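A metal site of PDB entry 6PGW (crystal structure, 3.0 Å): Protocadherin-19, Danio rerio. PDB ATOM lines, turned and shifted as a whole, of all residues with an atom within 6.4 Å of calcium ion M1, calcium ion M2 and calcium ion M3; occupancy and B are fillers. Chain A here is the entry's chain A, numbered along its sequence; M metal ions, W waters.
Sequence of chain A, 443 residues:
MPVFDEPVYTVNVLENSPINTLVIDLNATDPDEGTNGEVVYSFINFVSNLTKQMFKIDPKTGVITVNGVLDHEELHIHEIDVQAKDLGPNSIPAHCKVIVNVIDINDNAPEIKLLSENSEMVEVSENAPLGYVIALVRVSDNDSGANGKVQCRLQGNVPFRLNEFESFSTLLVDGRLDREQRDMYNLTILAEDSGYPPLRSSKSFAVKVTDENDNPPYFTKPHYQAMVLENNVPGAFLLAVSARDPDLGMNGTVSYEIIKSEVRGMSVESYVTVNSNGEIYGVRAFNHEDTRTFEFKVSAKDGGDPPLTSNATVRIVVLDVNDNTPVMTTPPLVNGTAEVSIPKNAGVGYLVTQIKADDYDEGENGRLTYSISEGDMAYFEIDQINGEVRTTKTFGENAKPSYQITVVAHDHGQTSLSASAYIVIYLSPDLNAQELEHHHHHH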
ATOM      1  N   GLU A  15       8.255  18.386 -31.254  1.00  0.00           N
ATOM      2  CA  GLU A  15       9.241  19.474 -31.320  1.00  0.00           C
ATOM      3  C   GLU A  15      10.609  19.078 -30.733  1.00  0.00           C
ATOM      4  O   GLU A  15      10.692  18.413 -29.736  1.00  0.00           O
ATOM      5  CB  GLU A  15       8.646  20.688 -30.582  1.00  0.00           C
ATOM      6  CG  GLU A  15       9.594  21.790 -30.199  1.00  0.00           C
ATOM      7  CD  GLU A  15       8.859  23.111 -29.935  1.00  0.00           C
ATOM      8  OE1 GLU A  15       7.882  23.191 -29.131  1.00  0.00           O
ATOM      9  OE2 GLU A  15       9.257  24.099 -30.548  1.00  0.00           O
ATOM     10  N   ASN A  16      11.667  19.470 -31.395  1.00  0.00           N
ATOM     11  CA  ASN A  16      13.030  19.159 -30.968  1.00  0.00           C
ATOM     12  C   ASN A  16      13.358  17.671 -30.824  1.00  0.00           C
ATOM     13  O   ASN A  16      14.266  17.320 -30.125  1.00  0.00           O
ATOM     14  CB  ASN A  16      13.374  19.932 -29.676  1.00  0.00           C
ATOM     15  CG  ASN A  16      13.028  21.402 -29.766  1.00  0.00           C
ATOM     16  OD1 ASN A  16      13.067  22.007 -30.857  1.00  0.00           O
ATOM     17  ND2 ASN A  16      12.696  22.000 -28.645  1.00  0.00           N
ATOM     18  N   LEU A  70      12.971  20.493 -35.305  1.00  0.00           N
ATOM     19  CA  LEU A  70      11.611  20.798 -35.566  1.00  0.00           C
ATOM     20  C   LEU A  70      11.168  21.828 -34.558  1.00  0.00           C
ATOM     21  O   LEU A  70      10.808  21.480 -33.455  1.00  0.00           O
ATOM     22  CB  LEU A  70      10.757  19.516 -35.484  1.00  0.00           C
ATOM     23  CG  LEU A  70      11.033  18.493 -36.600  1.00  0.00           C
ATOM     24  CD1 LEU A  70      10.509  17.120 -36.233  1.00  0.00           C
ATOM     25  CD2 LEU A  70      10.431  18.963 -37.924  1.00  0.00           C
ATOM     26  N   ASP A  71      11.209  23.101 -34.938  1.00  0.00           N
ATOM     27  CA  ASP A  71      10.778  24.205 -34.054  1.00  0.00           C
ATOM     28  C   ASP A  71       9.295  24.654 -34.248  1.00  0.00           C
ATOM     29  O   ASP A  71       8.986  25.414 -35.139  1.00  0.00           O
ATOM     30  CB  ASP A  71      11.721  25.397 -34.252  1.00  0.00           C
ATOM     31  CG  ASP A  71      11.490  26.512 -33.244  1.00  0.00           C
ATOM     32  OD1 ASP A  71      10.898  26.244 -32.165  1.00  0.00           O
ATOM     33  OD2 ASP A  71      11.905  27.673 -33.512  1.00  0.00           O
ATOM     34  N   HIS A  72       8.392  24.238 -33.345  1.00  0.00           N
ATOM     35  CA  HIS A  72       6.983  24.767 -33.329  1.00  0.00           C
ATOM     36  C   HIS A  72       6.816  26.290 -33.486  1.00  0.00           C
ATOM     37  O   HIS A  72       5.802  26.756 -34.056  1.00  0.00           O
ATOM     38  CB  HIS A  72       6.219  24.333 -32.054  1.00  0.00           C
ATOM     39  CG  HIS A  72       4.754  24.709 -32.079  1.00  0.00           C
ATOM     40  ND1 HIS A  72       3.789  23.923 -32.686  1.00  0.00           N
ATOM     41  CD2 HIS A  72       4.097  25.785 -31.578  1.00  0.00           C
ATOM     42  CE1 HIS A  72       2.608  24.505 -32.556  1.00  0.00           C
ATOM     43  NE2 HIS A  72       2.767  25.629 -31.886  1.00  0.00           N
ATOM     44  N   GLU A  73       7.741  27.051 -32.945  1.00  0.00           N
ATOM     45  CA  GLU A  73       7.657  28.499 -33.025  1.00  0.00           C
ATOM     46  C   GLU A  73       8.034  28.976 -34.454  1.00  0.00           C
ATOM     47  O   GLU A  73       7.627  30.057 -34.882  1.00  0.00           O
ATOM     48  CB  GLU A  73       8.528  29.128 -31.938  1.00  0.00           C
ATOM     49  CG  GLU A  73       7.971  28.938 -30.519  1.00  0.00           C
ATOM     50  CD  GLU A  73       8.159  27.547 -29.941  1.00  0.00           C
ATOM     51  OE1 GLU A  73       7.174  26.979 -29.408  1.00  0.00           O
ATOM     52  OE2 GLU A  73       9.308  26.999 -29.980  1.00  0.00           O
ATOM     53  N   GLU A  74       8.758  28.144 -35.178  1.00  0.00           N
ATOM     54  CA  GLU A  74       9.201  28.430 -36.543  1.00  0.00           C
ATOM     55  C   GLU A  74       8.146  27.880 -37.494  1.00  0.00           C
ATOM     56  O   GLU A  74       7.372  28.643 -38.067  1.00  0.00           O
ATOM     57  CB  GLU A  74      10.565  27.765 -36.756  1.00  0.00           C
ATOM     58  CG  GLU A  74      11.285  27.945 -38.081  1.00  0.00           C
ATOM     59  CD  GLU A  74      12.492  26.977 -38.199  1.00  0.00           C
ATOM     60  OE1 GLU A  74      12.329  25.755 -37.872  1.00  0.00           O
ATOM     61  OE2 GLU A  74      13.611  27.433 -38.584  1.00  0.00           O
ATOM     62  N   ILE A 103       4.237  19.007 -32.624  1.00  0.00           N
ATOM     63  CA  ILE A 103       3.577  19.202 -31.377  1.00  0.00           C
ATOM     64  C   ILE A 103       4.429  20.104 -30.519  1.00  0.00           C
ATOM     65  O   ILE A 103       5.609  19.833 -30.315  1.00  0.00           O
ATOM     66  CB  ILE A 103       3.328  17.863 -30.664  1.00  0.00           C
ATOM     67  CG1 ILE A 103       2.049  17.159 -31.221  1.00  0.00           C
ATOM     68  CG2 ILE A 103       3.117  18.088 -29.184  1.00  0.00           C
ATOM     69  CD1 ILE A 103       1.879  17.106 -32.751  1.00  0.00           C
ATOM     70  N   ASP A 104       3.816  21.199 -30.064  1.00  0.00           N
ATOM     71  CA  ASP A 104       4.448  22.221 -29.190  1.00  0.00           C
ATOM     72  C   ASP A 104       4.803  21.644 -27.851  1.00  0.00           C
ATOM     73  O   ASP A 104       3.984  21.012 -27.221  1.00  0.00           O
ATOM     74  CB  ASP A 104       3.486  23.370 -28.939  1.00  0.00           C
ATOM     75  CG  ASP A 104       4.081  24.441 -28.080  1.00  0.00           C
ATOM     76  OD1 ASP A 104       5.306  24.694 -28.194  1.00  0.00           O
ATOM     77  OD2 ASP A 104       3.321  25.050 -27.304  1.00  0.00           O
ATOM     78  N   ILE A 105       6.037  21.898 -27.405  1.00  0.00           N
ATOM     79  CA  ILE A 105       6.454  21.595 -26.025  1.00  0.00           C
ATOM     80  C   ILE A 105       7.003  22.866 -25.342  1.00  0.00           C
ATOM     81  O   ILE A 105       7.200  23.910 -26.012  1.00  0.00           O
ATOM     82  CB  ILE A 105       7.445  20.391 -25.986  1.00  0.00           C
ATOM     83  CG1 ILE A 105       8.786  20.753 -26.590  1.00  0.00           C
ATOM     84  CG2 ILE A 105       6.869  19.195 -26.739  1.00  0.00           C
ATOM     85  CD1 ILE A 105       9.696  19.575 -26.746  1.00  0.00           C
ATOM     86  N   ASN A 106       7.199  22.796 -24.015  1.00  0.00           N
ATOM     87  CA  ASN A 106       7.459  23.942 -23.160  1.00  0.00           C
ATOM     88  C   ASN A 106       8.983  24.204 -23.085  1.00  0.00           C
ATOM     89  O   ASN A 106       9.638  23.997 -22.059  1.00  0.00           O
ATOM     90  CB  ASN A 106       6.848  23.699 -21.767  1.00  0.00           C
ATOM     91  CG  ASN A 106       6.706  24.968 -20.952  1.00  0.00           C
ATOM     92  OD1 ASN A 106       6.680  26.053 -21.512  1.00  0.00           O
ATOM     93  ND2 ASN A 106       6.598  24.834 -19.612  1.00  0.00           N
ATOM     94  N   ASP A 107       9.533  24.658 -24.210  1.00  0.00           N
ATOM     95  CA  ASP A 107      10.987  24.872 -24.353  1.00  0.00           C
ATOM     96  C   ASP A 107      11.412  26.370 -24.295  1.00  0.00           C
ATOM     97  O   ASP A 107      12.578  26.655 -24.182  1.00  0.00           O
ATOM     98  CB  ASP A 107      11.547  24.139 -25.617  1.00  0.00           C
ATOM     99  CG  ASP A 107      10.908  24.601 -26.944  1.00  0.00           C
ATOM    100  OD1 ASP A 107       9.726  25.118 -26.971  1.00  0.00           O
ATOM    101  OD2 ASP A 107      11.591  24.406 -27.995  1.00  0.00           O
ATOM    102  N   ASN A 108      10.435  27.290 -24.310  1.00  0.00           N
ATOM    103  CA  ASN A 108      10.638  28.728 -24.067  1.00  0.00           C
ATOM    104  C   ASN A 108       9.982  29.136 -22.741  1.00  0.00           C
ATOM    105  O   ASN A 108       8.761  29.069 -22.581  1.00  0.00           O
ATOM    106  CB  ASN A 108      10.002  29.553 -25.207  1.00  0.00           C
ATOM    107  CG  ASN A 108      10.587  29.259 -26.570  1.00  0.00           C
ATOM    108  OD1 ASN A 108      11.507  29.913 -26.992  1.00  0.00           O
ATOM    109  ND2 ASN A 108       9.992  28.311 -27.283  1.00  0.00           N
ATOM    110  N   ALA A 109      10.779  29.627 -21.806  1.00  0.00           N
ATOM    111  CA  ALA A 109      10.258  30.145 -20.541  1.00  0.00           C
ATOM    112  C   ALA A 109       9.967  31.628 -20.686  1.00  0.00           C
ATOM    113  O   ALA A 109      10.250  32.193 -21.713  1.00  0.00           O
ATOM    114  CB  ALA A 109      11.279  29.891 -19.437  1.00  0.00           C
ATOM    115  N   PRO A 110       9.370  32.263 -19.659  1.00  0.00           N
ATOM    116  CA  PRO A 110       8.973  33.642 -19.843  1.00  0.00           C
ATOM    117  C   PRO A 110      10.140  34.647 -20.058  1.00  0.00           C
ATOM    118  O   PRO A 110      11.307  34.385 -19.710  1.00  0.00           O
ATOM    119  CB  PRO A 110       8.224  33.958 -18.547  1.00  0.00           C
ATOM    120  CG  PRO A 110       7.661  32.657 -18.133  1.00  0.00           C
ATOM    121  CD  PRO A 110       8.738  31.682 -18.462  1.00  0.00           C
ATOM    122  N   ASP A 141       5.980  34.544 -23.482  1.00  0.00           N
ATOM    123  CA  ASP A 141       6.451  33.154 -23.645  1.00  0.00           C
ATOM    124  C   ASP A 141       6.131  32.822 -25.080  1.00  0.00           C
ATOM    125  O   ASP A 141       5.038  33.134 -25.564  1.00  0.00           O
ATOM    126  CB  ASP A 141       5.707  32.188 -22.690  1.00  0.00           C
ATOM    127  CG  ASP A 141       6.378  30.818 -22.582  1.00  0.00           C
ATOM    128  OD1 ASP A 141       6.529  30.118 -23.610  1.00  0.00           O
ATOM    129  OD2 ASP A 141       6.715  30.444 -21.464  1.00  0.00           O
ATOM    130  N   ASN A 142       7.075  32.252 -25.794  1.00  0.00           N
ATOM    131  CA  ASN A 142       6.961  32.125 -27.233  1.00  0.00           C
ATOM    132  C   ASN A 142       6.277  30.848 -27.617  1.00  0.00           C
ATOM    133  O   ASN A 142       6.035  30.626 -28.798  1.00  0.00           O
ATOM    134  CB  ASN A 142       8.332  32.235 -27.885  1.00  0.00           C
ATOM    135  CG  ASN A 142       8.918  33.637 -27.765  1.00  0.00           C
ATOM    136  OD1 ASN A 142       8.683  34.338 -26.775  1.00  0.00           O
ATOM    137  ND2 ASN A 142       9.651  34.056 -28.766  1.00  0.00           N
ATOM    138  N   ASP A 143       5.935  30.000 -26.645  1.00  0.00           N
ATOM    139  CA  ASP A 143       5.160  28.784 -26.936  1.00  0.00           C
ATOM    140  C   ASP A 143       3.683  29.111 -27.104  1.00  0.00           C
ATOM    141  O   ASP A 143       3.237  30.256 -26.922  1.00  0.00           O
ATOM    142  CB  ASP A 143       5.320  27.726 -25.834  1.00  0.00           C
ATOM    143  CG  ASP A 143       6.765  27.375 -25.540  1.00  0.00           C
ATOM    144  OD1 ASP A 143       7.487  26.990 -26.491  1.00  0.00           O
ATOM    145  OD2 ASP A 143       7.155  27.462 -24.338  1.00  0.00           O
ATOM    146  N   SER A 144       2.928  28.058 -27.429  1.00  0.00           N
ATOM    147  CA  SER A 144       1.474  28.093 -27.530  1.00  0.00           C
ATOM    148  C   SER A 144       0.801  27.415 -26.359  1.00  0.00           C
ATOM    149  O   SER A 144       1.400  26.600 -25.683  1.00  0.00           O
ATOM    150  CB  SER A 144       1.062  27.407 -28.823  1.00  0.00           C
ATOM    151  OG  SER A 144       1.895  27.845 -29.885  1.00  0.00           O
ATOM    152  N   ALA A 146      -1.208  26.578 -22.797  1.00  0.00           N
ATOM    153  CA  ALA A 146      -0.743  26.662 -21.405  1.00  0.00           C
ATOM    154  C   ALA A 146       0.745  26.986 -21.320  1.00  0.00           C
ATOM    155  O   ALA A 146       1.173  27.718 -20.438  1.00  0.00           O
ATOM    156  CB  ALA A 146      -1.010  25.348 -20.701  1.00  0.00           C
ATOM    157  N   ASN A 147       1.517  26.394 -22.230  1.00  0.00           N
ATOM    158  CA  ASN A 147       2.938  26.616 -22.314  1.00  0.00           C
ATOM    159  C   ASN A 147       3.251  28.048 -22.683  1.00  0.00           C
ATOM    160  O   ASN A 147       4.344  28.548 -22.382  1.00  0.00           O
ATOM    161  CB  ASN A 147       3.562  25.683 -23.340  1.00  0.00           C
ATOM    162  CG  ASN A 147       3.562  24.250 -22.882  1.00  0.00           C
ATOM    163  OD1 ASN A 147       3.330  23.971 -21.724  1.00  0.00           O
ATOM    164  ND2 ASN A 147       3.868  23.347 -23.778  1.00  0.00           N
ATOM    165  N   GLY A 148       2.294  28.715 -23.327  1.00  0.00           N
ATOM    166  CA  GLY A 148       2.386  30.135 -23.605  1.00  0.00           C
ATOM    167  C   GLY A 148       1.866  31.085 -22.528  1.00  0.00           C
ATOM    168  O   GLY A 148       2.309  32.205 -22.479  1.00  0.00           O
ATOM    169  N   LYS A 149       0.895  30.647 -21.722  1.00  0.00           N
ATOM    170  CA  LYS A 149       0.231  31.556 -20.739  1.00  0.00           C
ATOM    171  C   LYS A 149       1.090  31.901 -19.548  1.00  0.00           C
ATOM    172  O   LYS A 149       1.782  31.042 -18.991  1.00  0.00           O
ATOM    173  CB  LYS A 149      -1.072  30.939 -20.216  1.00  0.00           C
ATOM    174  CG  LYS A 149      -2.284  31.262 -21.067  1.00  0.00           C
ATOM    175  CD  LYS A 149      -3.184  30.028 -21.216  1.00  0.00           C
ATOM    176  CE  LYS A 149      -4.165  30.140 -22.381  1.00  0.00           C
ATOM    177  NZ  LYS A 149      -4.765  28.818 -22.709  1.00  0.00           N
ATOM    178  N   VAL A 150       1.016  33.153 -19.106  1.00  0.00           N
ATOM    179  CA  VAL A 150       1.883  33.608 -18.017  1.00  0.00           C
ATOM    180  C   VAL A 150       1.267  34.652 -17.070  1.00  0.00           C
ATOM    181  O   VAL A 150       0.555  35.570 -17.500  1.00  0.00           O
ATOM    182  CB  VAL A 150       3.191  34.175 -18.590  1.00  0.00           C
ATOM    183  CG1 VAL A 150       3.796  33.223 -19.630  1.00  0.00           C
ATOM    184  CG2 VAL A 150       2.953  35.533 -19.230  1.00  0.00           C
ATOM    185  N   ASP A 193       5.466  30.427 -16.560  1.00  0.00           N
ATOM    186  CA  ASP A 193       4.467  29.991 -17.573  1.00  0.00           C
ATOM    187  C   ASP A 193       3.531  28.976 -16.998  1.00  0.00           C
ATOM    188  O   ASP A 193       3.699  28.576 -15.889  1.00  0.00           O
ATOM    189  CB  ASP A 193       5.110  29.558 -18.935  1.00  0.00           C
ATOM    190  CG  ASP A 193       5.976  28.271 -18.867  1.00  0.00           C
ATOM    191  OD1 ASP A 193       5.838  27.458 -17.928  1.00  0.00           O
ATOM    192  OD2 ASP A 193       6.774  28.075 -19.836  1.00  0.00           O
ATOM    193  N   SER A 194       2.493  28.604 -17.724  1.00  0.00           N
ATOM    194  CA  SER A 194       1.494  27.683 -17.190  1.00  0.00           C
ATOM    195  C   SER A 194       1.609  26.262 -17.724  1.00  0.00           C
ATOM    196  O   SER A 194       0.637  25.502 -17.691  1.00  0.00           O
ATOM    197  CB  SER A 194       0.087  28.237 -17.421  1.00  0.00           C
ATOM    198  OG  SER A 194       0.057  29.638 -17.122  1.00  0.00           O
ATOM    199  N   GLY A 195       2.813  25.886 -18.184  1.00  0.00           N
ATOM    200  CA  GLY A 195       3.112  24.487 -18.539  1.00  0.00           C
ATOM    201  C   GLY A 195       3.221  23.585 -17.309  1.00  0.00           C
ATOM    202  O   GLY A 195       3.083  24.052 -16.194  1.00  0.00           O
ATOM    203  N   LEU A 199       7.471  26.712 -16.127  1.00  0.00           N
ATOM    204  CA  LEU A 199       8.828  27.265 -16.178  1.00  0.00           C
ATOM    205  C   LEU A 199       8.816  28.663 -15.697  1.00  0.00           C
ATOM    206  O   LEU A 199       7.957  29.433 -16.106  1.00  0.00           O
ATOM    207  CB  LEU A 199       9.371  27.215 -17.599  1.00  0.00           C
ATOM    208  CG  LEU A 199      10.067  25.900 -17.907  1.00  0.00           C
ATOM    209  CD1 LEU A 199       9.997  25.564 -19.386  1.00  0.00           C
ATOM    210  CD2 LEU A 199      11.510  25.966 -17.452  1.00  0.00           C
HETATM  211 CA    CA M   1       7.571  25.193 -27.928  1.00  0.00          CA
HETATM  212 CA    CA M   2      11.009  25.419 -30.016  1.00  0.00          CA
HETATM  213 CA    CA M   3       6.647  28.255 -22.202  1.00  0.00          CA
HETATM  214  O   HOH W   1      12.230  27.404 -30.003  1.00  0.00           O
HETATM  215  O   HOH W   2      13.171  24.804 -30.587  1.00  0.00           O
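Within 4 Å of calcium ion M1: Glu 15, Glu 73, Asp 104, Ile 105, Asp 107, Asn 108 and Asp 143.
Calcium ion M2 is bound by the side-chain carboxylate (OE2) of Glu 15 (2.3 Å), the side-chain carboxylate (OD1) of Asp 71 (2.3 Å), water W2 (2.3 Å), the side-chain carboxylate (OE2) of Glu 73 (2.3 Å), water W1 (2.3 Å) and the side-chain carboxylate (OD2) of Asp 107 (2.3 Å). Calcium ion M2 has six donor atoms within binding distance.
Calcium ion M1 is bound by OD1 of Asp 143, at 2.3 Å. OD1 of Asp 104 binds calcium ion M1 (2.3 Å). Calcium ion M1 is bound by O of Ile 105 (2.3 Å). Calcium ion M1 is bound by OE1 of Glu 73, 2.4 Å away. OE1 of Glu 15 binds calcium ion M1 (2.4 Å). OD1 of Asp 107 is bound to calcium ion M1. Calcium ion M1 has six donor atoms within binding distance.
The side-chain carboxylate (OD2) of Asp 104 is in hydrogen-bond range of the backbone NH (N) of Ser 144, at 3.0 Å. The side-chain carboxylate (OD1) of Asp 193 sits close to the backbone NH (N) of Gly 195 (3.4 Å). The side-chain carboxylate (OD2) of Asp 107 sits close to the side-chain amide nitrogen (ND2) of Asn 16, at 2.7 Å. The backbone NH of Glu 15 is in hydrogen-bond range of the backbone carbonyl oxygen of Ile 103. The side-chain carboxylate (OE2) of Glu 73 sits close to the side-chain amide nitrogen (ND2) of Asn 108 (3.1 Å). OE2 of Glu 15 sits close to N of His 72 (2.9 Å). The side-chain amide nitrogen of Asn 108 lies close to the side-chain carboxylate of Asp 107 (3.2 Å). The side-chain carboxylate (OD1) of Asp 193 lies within hydrogen-bond range of the backbone NH (N) of Leu 199, 2.5 Å away.
Four residues have an atom within 4 Å of calcium ion M2: Glu 15, Asp 71, Glu 73 and Asp 107. The nearest printed residue that does not touch calcium ion M2 is Asn 16 (4.1 Å).
Six residues have an atom within 4 Å of calcium ion M3: Asn 106, Asn 108, Asp 141, Asp 143, Asn 147 and Asp 193.
Calcium ion M3 is bound by O of Asn 108, OD1 of Asn 106, OD2 of Asp 141, O of Asn 147, OD2 of Asp 143, OD1 of Asp 141 and OD2 of Asp 193.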
